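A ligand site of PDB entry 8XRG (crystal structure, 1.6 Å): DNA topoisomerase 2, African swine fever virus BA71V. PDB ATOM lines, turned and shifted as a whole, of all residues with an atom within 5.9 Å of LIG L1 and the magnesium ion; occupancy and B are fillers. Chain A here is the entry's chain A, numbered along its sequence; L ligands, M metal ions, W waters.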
ATOM      1  N   GLU A  60      16.229 -36.853   4.254  1.00  0.00           N
ATOM      2  CA  GLU A  60      16.734 -35.503   4.455  1.00  0.00           C
ATOM      3  C   GLU A  60      17.071 -35.249   5.921  1.00  0.00           C
ATOM      4  O   GLU A  60      18.071 -34.593   6.226  1.00  0.00           O
ATOM      5  CB  GLU A  60      15.709 -34.467   3.984  1.00  0.00           C
ATOM      6  CG  GLU A  60      15.459 -34.428   2.461  1.00  0.00           C
ATOM      7  CD  GLU A  60      16.661 -34.027   1.594  1.00  0.00           C
ATOM      8  OE1 GLU A  60      17.778 -33.778   2.128  1.00  0.00           O
ATOM      9  OE2 GLU A  60      16.483 -33.973   0.351  1.00  0.00           O
ATOM     10  N   LEU A  61      16.263 -35.773   6.846  1.00  0.00           N
ATOM     11  CA  LEU A  61      16.605 -35.598   8.255  1.00  0.00           C
ATOM     12  C   LEU A  61      17.826 -36.425   8.631  1.00  0.00           C
ATOM     13  O   LEU A  61      18.677 -35.969   9.403  1.00  0.00           O
ATOM     14  CB  LEU A  61      15.431 -35.991   9.158  1.00  0.00           C
ATOM     15  CG  LEU A  61      14.428 -34.899   9.531  1.00  0.00           C
ATOM     16  CD1 LEU A  61      14.096 -34.023   8.362  1.00  0.00           C
ATOM     17  CD2 LEU A  61      13.175 -35.540  10.148  1.00  0.00           C
ATOM     18  N   VAL A  63      20.330 -37.424   6.682  1.00  0.00           N
ATOM     19  CA  VAL A  63      21.570 -36.855   6.132  1.00  0.00           C
ATOM     20  C   VAL A  63      21.930 -35.571   6.862  1.00  0.00           C
ATOM     21  O   VAL A  63      23.107 -35.286   7.065  1.00  0.00           O
ATOM     22  CB  VAL A  63      21.464 -36.632   4.600  1.00  0.00           C
ATOM     23  CG1 VAL A  63      22.755 -36.007   4.033  1.00  0.00           C
ATOM     24  CG2 VAL A  63      21.198 -37.978   3.882  1.00  0.00           C
ATOM     25  N   ASN A  64      20.946 -34.787   7.307  1.00  0.00           N
ATOM     26  CA  ASN A  64      21.289 -33.594   8.094  1.00  0.00           C
ATOM     27  C   ASN A  64      22.022 -33.974   9.364  1.00  0.00           C
ATOM     28  O   ASN A  64      22.962 -33.287   9.778  1.00  0.00           O
ATOM     29  CB  ASN A  64      20.028 -32.799   8.434  1.00  0.00           C
ATOM     30  CG  ASN A  64      19.573 -31.947   7.283  1.00  0.00           C
ATOM     31  OD1 ASN A  64      20.346 -31.689   6.354  1.00  0.00           O
ATOM     32  ND2 ASN A  64      18.360 -31.446   7.369  1.00  0.00           N
ATOM     33  N   ALA A  65      21.617 -35.072   9.995  1.00  0.00           N
ATOM     34  CA  ALA A  65      22.274 -35.498  11.231  1.00  0.00           C
ATOM     35  C   ALA A  65      23.653 -36.039  10.940  1.00  0.00           C
ATOM     36  O   ALA A  65      24.610 -35.766  11.698  1.00  0.00           O
ATOM     37  CB  ALA A  65      21.396 -36.553  11.927  1.00  0.00           C
ATOM     38  N   ASP A  67      25.495 -35.106   8.392  1.00  0.00           N
ATOM     39  CA  ASP A  67      26.301 -33.907   8.105  1.00  0.00           C
ATOM     40  C   ASP A  67      26.820 -33.241   9.358  1.00  0.00           C
ATOM     41  O   ASP A  67      27.949 -32.707   9.374  1.00  0.00           O
ATOM     42  CB  ASP A  67      25.512 -32.859   7.314  1.00  0.00           C
ATOM     43  CG  ASP A  67      25.201 -33.257   5.905  1.00  0.00           C
ATOM     44  OD1 ASP A  67      25.849 -34.196   5.363  1.00  0.00           O
ATOM     45  OD2 ASP A  67      24.256 -32.645   5.325  1.00  0.00           O
ATOM     46  N   HIS A  68      25.982 -33.151  10.369  1.00  0.00           N
ATOM     47  CA  HIS A  68      26.425 -32.529  11.614  1.00  0.00           C
ATOM     48  C   HIS A  68      27.497 -33.392  12.268  1.00  0.00           C
ATOM     49  O   HIS A  68      28.451 -32.863  12.832  1.00  0.00           O
ATOM     50  CB  HIS A  68      25.231 -32.333  12.560  1.00  0.00           C
ATOM     51  CG  HIS A  68      25.393 -31.184  13.521  1.00  0.00           C
ATOM     52  ND1 HIS A  68      25.680 -29.899  13.098  1.00  0.00           N
ATOM     53  CD2 HIS A  68      25.257 -31.122  14.866  1.00  0.00           C
ATOM     54  CE1 HIS A  68      25.737 -29.095  14.155  1.00  0.00           C
ATOM     55  NE2 HIS A  68      25.484 -29.812  15.235  1.00  0.00           N
ATOM     56  N   ASN A  95      20.007 -35.666  17.283  1.00  0.00           N
ATOM     57  CA  ASN A  95      21.442 -35.820  17.461  1.00  0.00           C
ATOM     58  C   ASN A  95      21.933 -34.856  18.533  1.00  0.00           C
ATOM     59  O   ASN A  95      21.322 -33.809  18.769  1.00  0.00           O
ATOM     60  CB  ASN A  95      22.205 -35.619  16.147  1.00  0.00           C
ATOM     61  CG  ASN A  95      21.900 -34.291  15.488  1.00  0.00           C
ATOM     62  OD1 ASN A  95      20.987 -34.206  14.668  1.00  0.00           O
ATOM     63  ND2 ASN A  95      22.640 -33.239  15.845  1.00  0.00           N
ATOM     64  N   PRO A  98      26.642 -29.504  19.099  1.00  0.00           N
ATOM     65  CA  PRO A  98      26.119 -28.140  19.210  1.00  0.00           C
ATOM     66  C   PRO A  98      24.761 -27.989  18.542  1.00  0.00           C
ATOM     67  O   PRO A  98      24.523 -28.518  17.450  1.00  0.00           O
ATOM     68  CB  PRO A  98      27.194 -27.307  18.510  1.00  0.00           C
ATOM     69  CG  PRO A  98      28.462 -28.095  18.724  1.00  0.00           C
ATOM     70  CD  PRO A  98      28.057 -29.542  18.671  1.00  0.00           C
ATOM     71  N   GLY A  99      23.853 -27.308  19.227  1.00  0.00           N
ATOM     72  CA  GLY A  99      22.543 -27.056  18.666  1.00  0.00           C
ATOM     73  C   GLY A  99      22.590 -25.984  17.579  1.00  0.00           C
ATOM     74  O   GLY A  99      23.579 -25.270  17.392  1.00  0.00           O
ATOM     75  N   ILE A 100      21.495 -25.907  16.834  1.00  0.00           N
ATOM     76  CA  ILE A 100      21.315 -24.759  15.950  1.00  0.00           C
ATOM     77  C   ILE A 100      21.304 -23.480  16.790  1.00  0.00           C
ATOM     78  O   ILE A 100      20.605 -23.430  17.826  1.00  0.00           O
ATOM     79  CB  ILE A 100      20.024 -24.891  15.140  1.00  0.00           C
ATOM     80  CG1 ILE A 100      20.028 -26.231  14.374  1.00  0.00           C
ATOM     81  CG2 ILE A 100      19.819 -23.687  14.263  1.00  0.00           C
ATOM     82  CD1 ILE A 100      18.771 -26.485  13.565  1.00  0.00           C
ATOM     83  N   ALA A 122      16.360 -22.176   9.436  1.00  0.00           N
ATOM     84  CA  ALA A 122      16.782 -23.522   9.050  1.00  0.00           C
ATOM     85  C   ALA A 122      15.610 -24.391   8.618  1.00  0.00           C
ATOM     86  O   ALA A 122      15.759 -25.211   7.709  1.00  0.00           O
ATOM     87  CB  ALA A 122      17.511 -24.190  10.222  1.00  0.00           C
ATOM     88  N   SER A 123      14.441 -24.205   9.236  1.00  0.00           N
ATOM     89  CA  SER A 123      13.335 -25.129   8.993  1.00  0.00           C
ATOM     90  C   SER A 123      12.249 -24.583   8.087  1.00  0.00           C
ATOM     91  O   SER A 123      11.490 -25.379   7.521  1.00  0.00           O
ATOM     92  CB  SER A 123      12.713 -25.561  10.338  1.00  0.00           C
ATOM     93  OG  SER A 123      12.262 -24.419  11.057  1.00  0.00           O
ATOM     94  N   ALA A 128      17.915 -21.932   2.177  1.00  0.00           N
ATOM     95  CA  ALA A 128      18.589 -21.334   3.323  1.00  0.00           C
ATOM     96  C   ALA A 128      19.280 -22.405   4.152  1.00  0.00           C
ATOM     97  O   ALA A 128      18.725 -23.476   4.405  1.00  0.00           O
ATOM     98  CB  ALA A 128      17.598 -20.544   4.192  1.00  0.00           C
ATOM     99  N   GLY A 129      20.485 -22.098   4.603  1.00  0.00           N
ATOM    100  CA  GLY A 129      21.236 -23.044   5.416  1.00  0.00           C
ATOM    101  C   GLY A 129      22.690 -22.624   5.493  1.00  0.00           C
ATOM    102  O   GLY A 129      23.069 -21.560   4.999  1.00  0.00           O
ATOM    103  N   THR A 130      23.500 -23.486   6.089  1.00  0.00           N
ATOM    104  CA  THR A 130      24.935 -23.203   6.224  1.00  0.00           C
ATOM    105  C   THR A 130      25.776 -23.755   5.074  1.00  0.00           C
ATOM    106  O   THR A 130      27.007 -23.640   5.114  1.00  0.00           O
ATOM    107  CB  THR A 130      25.471 -23.784   7.535  1.00  0.00           C
ATOM    108  OG1 THR A 130      25.245 -25.188   7.592  1.00  0.00           O
ATOM    109  CG2 THR A 130      24.760 -23.126   8.695  1.00  0.00           C
ATOM    110  N   ASN A 131      25.139 -24.352   4.053  1.00  0.00           N
ATOM    111  CA  ASN A 131      25.847 -24.904   2.906  1.00  0.00           C
ATOM    112  C   ASN A 131      25.500 -24.186   1.603  1.00  0.00           C
ATOM    113  O   ASN A 131      25.830 -24.690   0.530  1.00  0.00           O
ATOM    114  CB  ASN A 131      25.535 -26.409   2.788  1.00  0.00           C
ATOM    115  CG  ASN A 131      25.996 -27.176   3.990  1.00  0.00           C
ATOM    116  OD1 ASN A 131      27.184 -27.182   4.305  1.00  0.00           O
ATOM    117  ND2 ASN A 131      25.059 -27.778   4.701  1.00  0.00           N
ATOM    118  N   ILE A 132      24.836 -23.033   1.677  1.00  0.00           N
ATOM    119  CA  ILE A 132      24.549 -22.279   0.455  1.00  0.00           C
ATOM    120  C   ILE A 132      25.837 -21.872  -0.222  1.00  0.00           C
ATOM    121  O   ILE A 132      26.029 -22.039  -1.437  1.00  0.00           O
ATOM    122  CB  ILE A 132      23.659 -21.071   0.791  1.00  0.00           C
ATOM    123  CG1 ILE A 132      22.275 -21.528   1.267  1.00  0.00           C
ATOM    124  CG2 ILE A 132      23.561 -20.111  -0.427  1.00  0.00           C
ATOM    125  CD1 ILE A 132      21.485 -22.365   0.250  1.00  0.00           C
ATOM    126  N   GLY A 141      26.650 -33.937   2.808  1.00  0.00           N
ATOM    127  CA  GLY A 141      25.675 -34.152   1.740  1.00  0.00           C
ATOM    128  C   GLY A 141      24.800 -32.934   1.492  1.00  0.00           C
ATOM    129  O   GLY A 141      24.412 -32.673   0.345  1.00  0.00           O
ATOM    130  N   GLY A 142      24.538 -32.155   2.539  1.00  0.00           N
ATOM    131  CA  GLY A 142      23.698 -30.980   2.385  1.00  0.00           C
ATOM    132  C   GLY A 142      24.322 -29.952   1.460  1.00  0.00           C
ATOM    133  O   GLY A 142      25.543 -29.734   1.453  1.00  0.00           O
ATOM    134  N   THR A 143      23.471 -29.310   0.661  1.00  0.00           N
ATOM    135  CA  THR A 143      23.946 -28.266  -0.224  1.00  0.00           C
ATOM    136  C   THR A 143      22.843 -27.282  -0.559  1.00  0.00           C
ATOM    137  O   THR A 143      23.093 -26.088  -0.659  1.00  0.00           O
ATOM    138  CB  THR A 143      24.557 -28.906  -1.499  1.00  0.00           C
ATOM    139  OG1 THR A 143      25.114 -27.886  -2.334  1.00  0.00           O
ATOM    140  CG2 THR A 143      23.554 -29.753  -2.279  1.00  0.00           C
ATOM    141  N   ASN A 144      21.604 -27.750  -0.740  1.00  0.00           N
ATOM    142  CA  ASN A 144      20.614 -26.888  -1.381  1.00  0.00           C
ATOM    143  C   ASN A 144      19.887 -25.954  -0.421  1.00  0.00           C
ATOM    144  O   ASN A 144      19.200 -25.042  -0.886  1.00  0.00           O
ATOM    145  CB  ASN A 144      19.578 -27.745  -2.130  1.00  0.00           C
ATOM    146  CG  ASN A 144      20.193 -28.569  -3.190  1.00  0.00           C
ATOM    147  OD1 ASN A 144      20.964 -28.074  -4.036  1.00  0.00           O
ATOM    148  ND2 ASN A 144      19.862 -29.822  -3.189  1.00  0.00           N
ATOM    149  N   GLY A 145      19.956 -26.186   0.879  1.00  0.00           N
ATOM    150  CA  GLY A 145      19.117 -25.416   1.786  1.00  0.00           C
ATOM    151  C   GLY A 145      17.632 -25.633   1.608  1.00  0.00           C
ATOM    152  O   GLY A 145      16.851 -24.717   1.868  1.00  0.00           O
ATOM    153  N   VAL A 146      17.214 -26.826   1.197  1.00  0.00           N
ATOM    154  CA  VAL A 146      15.780 -27.093   1.081  1.00  0.00           C
ATOM    155  C   VAL A 146      15.350 -28.346   1.816  1.00  0.00           C
ATOM    156  O   VAL A 146      14.149 -28.501   2.076  1.00  0.00           O
ATOM    157  CB  VAL A 146      15.303 -27.167  -0.394  1.00  0.00           C
ATOM    158  CG1 VAL A 146      15.736 -25.940  -1.209  1.00  0.00           C
ATOM    159  CG2 VAL A 146      15.792 -28.435  -1.067  1.00  0.00           C
ATOM    160  N   GLY A 147      16.261 -29.248   2.209  1.00  0.00           N
ATOM    161  CA  GLY A 147      15.846 -30.566   2.668  1.00  0.00           C
ATOM    162  C   GLY A 147      14.935 -30.527   3.883  1.00  0.00           C
ATOM    163  O   GLY A 147      13.929 -31.237   3.918  1.00  0.00           O
ATOM    164  N   LEU A 148      15.268 -29.709   4.874  1.00  0.00           N
ATOM    165  CA  LEU A 148      14.437 -29.659   6.074  1.00  0.00           C
ATOM    166  C   LEU A 148      13.099 -29.009   5.776  1.00  0.00           C
ATOM    167  O   LEU A 148      12.083 -29.351   6.397  1.00  0.00           O
ATOM    168  CB  LEU A 148      15.187 -28.896   7.171  1.00  0.00           C
ATOM    169  CG  LEU A 148      14.496 -28.780   8.536  1.00  0.00           C
ATOM    170  CD1 LEU A 148      14.052 -30.131   9.029  1.00  0.00           C
ATOM    171  CD2 LEU A 148      15.482 -28.168   9.525  1.00  0.00           C
ATOM    172  N   LYS A 149      13.087 -28.052   4.835  1.00  0.00           N
ATOM    173  CA  LYS A 149      11.822 -27.408   4.465  1.00  0.00           C
ATOM    174  C   LYS A 149      10.897 -28.393   3.773  1.00  0.00           C
ATOM    175  O   LYS A 149       9.681 -28.343   3.972  1.00  0.00           O
ATOM    176  CB  LYS A 149      12.062 -26.208   3.544  1.00  0.00           C
ATOM    177  CG  LYS A 149      12.413 -24.900   4.259  1.00  0.00           C
ATOM    178  CD  LYS A 149      13.711 -25.004   5.055  1.00  0.00           C
ATOM    179  CE  LYS A 149      14.924 -25.162   4.178  1.00  0.00           C
ATOM    180  NZ  LYS A 149      16.205 -24.886   4.947  1.00  0.00           N
ATOM    181  N   THR A 193      19.773 -31.423  18.827  1.00  0.00           N
ATOM    182  CA  THR A 193      18.782 -30.985  17.845  1.00  0.00           C
ATOM    183  C   THR A 193      17.858 -32.159  17.569  1.00  0.00           C
ATOM    184  O   THR A 193      18.336 -33.265  17.310  1.00  0.00           O
ATOM    185  CB  THR A 193      19.439 -30.522  16.537  1.00  0.00           C
ATOM    186  OG1 THR A 193      20.300 -29.412  16.809  1.00  0.00           O
ATOM    187  CG2 THR A 193      18.377 -30.097  15.492  1.00  0.00           C
ATOM    188  N   ILE A 195      14.179 -33.220  15.379  1.00  0.00           N
ATOM    189  CA  ILE A 195      13.015 -32.965  14.534  1.00  0.00           C
ATOM    190  C   ILE A 195      12.039 -34.108  14.724  1.00  0.00           C
ATOM    191  O   ILE A 195      12.436 -35.271  14.585  1.00  0.00           O
ATOM    192  CB  ILE A 195      13.399 -32.829  13.049  1.00  0.00           C
ATOM    193  CG1 ILE A 195      14.644 -31.951  12.857  1.00  0.00           C
ATOM    194  CG2 ILE A 195      12.158 -32.440  12.194  1.00  0.00           C
ATOM    195  CD1 ILE A 195      14.429 -30.477  13.104  1.00  0.00           C
HETATM  196  P1  LIG L   1      21.241 -28.206   3.840  1.00  0.00           P
HETATM  197  O1  LIG L   1      22.254 -27.226   4.342  1.00  0.00           O
HETATM  198  O2  LIG L   1      21.207 -28.176   2.358  1.00  0.00           O
HETATM  199  O3  LIG L   1      21.339 -29.567   4.430  1.00  0.00           O
HETATM  200  P2  LIG L   1      18.597 -28.203   5.110  1.00  0.00           P
HETATM  201  O4  LIG L   1      18.598 -29.693   4.994  1.00  0.00           O
HETATM  202  O5  LIG L   1      17.367 -27.420   4.723  1.00  0.00           O
HETATM  203  O6  LIG L   1      19.813 -27.584   4.266  1.00  0.00           O
HETATM  204  O7  LIG L   1      18.991 -27.810   6.612  1.00  0.00           O
HETATM  205  C1  LIG L   1      19.087 -26.394   6.874  1.00  0.00           C
HETATM  206  C2  LIG L   1      20.193 -26.090   7.875  1.00  0.00           C
HETATM  207  O8  LIG L   1      19.787 -26.452   9.193  1.00  0.00           O
HETATM  208  C3  LIG L   1      21.465 -26.876   7.611  1.00  0.00           C
HETATM  209  O9  LIG L   1      22.300 -26.170   6.698  1.00  0.00           O
HETATM  210  C4  LIG L   1      22.104 -26.993   8.993  1.00  0.00           C
HETATM  211  O10 LIG L   1      22.868 -25.811   9.256  1.00  0.00           O
HETATM  212  C5  LIG L   1      20.901 -26.963   9.930  1.00  0.00           C
HETATM  213  N1  LIG L   1      20.522 -28.319  10.371  1.00  0.00           N
HETATM  214  C6  LIG L   1      19.553 -29.104   9.859  1.00  0.00           C
HETATM  215  N2  LIG L   1      19.444 -30.282  10.523  1.00  0.00           N
HETATM  216  C7  LIG L   1      20.340 -30.217  11.532  1.00  0.00           C
HETATM  217  C8  LIG L   1      20.738 -31.139  12.611  1.00  0.00           C
HETATM  218  N3  LIG L   1      20.136 -32.352  12.750  1.00  0.00           N
HETATM  219  N4  LIG L   1      21.708 -30.703  13.423  1.00  0.00           N
HETATM  220  C9  LIG L   1      22.308 -29.507  13.298  1.00  0.00           C
HETATM  221  N5  LIG L   1      22.012 -28.612  12.331  1.00  0.00           N
HETATM  222  C10 LIG L   1      21.054 -28.937  11.436  1.00  0.00           C
HETATM  223  P1  LG2 L   2      19.509 -30.491   1.058  1.00  0.00           P
HETATM  224  O1  LG2 L   2      20.650 -30.474   0.088  1.00  0.00           O
HETATM  225  O2  LG2 L   2      19.024 -29.062   1.210  1.00  0.00           O
HETATM  226  O3  LG2 L   2      19.799 -31.025   2.415  1.00  0.00           O
HETATM  227  O4  LG2 L   2      18.319 -31.263   0.492  1.00  0.00           O
HETATM  228 MG    MG M   1      20.002 -31.112   4.348  1.00  0.00          MG
HETATM  229  O   HOH W   1      17.081 -31.865   9.963  1.00  0.00           O
HETATM  230  O   HOH W   2      23.530 -26.386  12.129  1.00  0.00           O
HETATM  231  O   HOH W   3      21.579 -32.533   4.063  1.00  0.00           O
HETATM  232  O   HOH W   4      23.334 -30.204   6.358  1.00  0.00           O
HETATM  233  O   HOH W   5      18.039 -34.113  11.393  1.00  0.00           O
HETATM  234  O   HOH W   6      23.070 -30.458   9.153  1.00  0.00           O
HETATM  235  O   HOH W   7      18.469 -34.910  14.080  1.00  0.00           O
HETATM  236  O   HOH W   8      18.546 -32.604   4.320  1.00  0.00           O
HETATM  237  O   HOH W   9      22.457 -24.876   3.050  1.00  0.00           O
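The magnesium ion is bound by O3 of LG2 L2, O3 of LIG L1, water W8, O4 of LIG L1, OD1 of Asn 64 and water W3.
One residue has an atom within 4 Å of the magnesium ion: Asn 64. The nearest printed residue that does not touch the magnesium ion is Glu 60 (4.1 Å).
ND1 of His 68 touches C9 of LIG L1 (3.4 Å). Ile 100 touches LIG L1. CB of Ala 122 touches O8 of LIG L1 (3.4 Å). Ala 128 touches LIG L1 (O to C1, 3.8 Å). Gly 129 touches LIG L1 (CA to O9, 3.5 Å). CA of Gly 142 touches O3 of LIG L1 (3.4 Å). Val 146 touches LIG L1. CB of Thr 193 touches N4 of LIG L1 (3.9 Å). Hydrophobic or aromatic side chains that line LIG L1: His 68, Ile 100, Ala 122 and Leu 148. The nearest printed residue that does not touch LIG L1 is Ala 65 (4.1 Å).
Water W3 lies within hydrogen-bond range of OD2 of Asp 67 (3.0 Å) and N of Gly 142 (3.3 Å). Water W8 lies within hydrogen-bond range of OE1 of Glu 60 (2.6 Å) and ND2 of Asn 64 (3.3 Å). Water W4 lies within hydrogen-bond range of OD2 of Asp 67 and ND2 of Asn 131. Water W1 bridges N2 of LIG L1 and ND2 of Asn 64. Water W5 bridges O of Leu 61 (2.8 Å) and N3 of LIG L1 (3.1 Å). Water W7 lies within hydrogen-bond range of the side-chain amide oxygen (OD1) of Asn 95 (2.7 Å) and a nitrogen (N3) of LIG L1 (3.3 Å).
The side-chain amino group (NZ) of Lys 149 lies within hydrogen-bond range of the backbone carbonyl oxygen (O) of Ala 128 (2.9 Å). O of Pro 98 lies within hydrogen-bond range of NE2 of His 68. The backbone carbonyl oxygen of Asn 95 is in hydrogen-bond range of the backbone NH of Thr 193, 2.8 Å away. N of Gly 142 is in hydrogen-bond range of OD2 of Asp 67, at 2.8 Å. ND2 of Asn 64 sits close to O of Glu 60 (3.4 Å). The backbone carbonyl oxygen (O) of Gly 145 lies within hydrogen-bond range of the backbone NH (N) of Ala 128, at 3.0 Å. The backbone carbonyl oxygen (O) of Gly 145 sits close to the side-chain amino group (NZ) of Lys 149, 3.2 Å away. The side-chain amino group (NZ) of Lys 149 is in hydrogen-bond range of the backbone carbonyl oxygen (O) of Ala 122 (2.8 Å).
An oxygen (O5) of LIG L1 is in hydrogen-bond range of the backbone NH (N) of Gly 147 (3.3 Å). An oxygen (O2) of LIG L1 lies within hydrogen-bond range of the backbone NH of Gly 145. The backbone NH (N) of Asn 144 lies within hydrogen-bond range of an oxygen (O2) of LIG L1 (3.2 Å). The side-chain amide oxygen (OD1) of Asn 95 sits at hydrogen-bond distance from a nitrogen (N3) of LIG L1, at 2.8 Å. O9 of LIG L1 is in hydrogen-bond range of N of Thr 130, 3.0 Å away. ND2 of Asn 131 is in hydrogen-bond range of O1 of LIG L1 (2.9 Å). The backbone NH of Thr 143 sits at hydrogen-bond distance from an oxygen (O2) of LIG L1. An oxygen (O10) of LIG L1 sits at hydrogen-bond distance from the side-chain hydroxyl (OG1) of Thr 130, at 3.0 Å. N of Leu 148 sits at hydrogen-bond distance from O5 of LIG L1 (3.1 Å). NZ of Lys 149 lies within salt-bridge range of O5 of LIG L1, at 2.8 Å.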
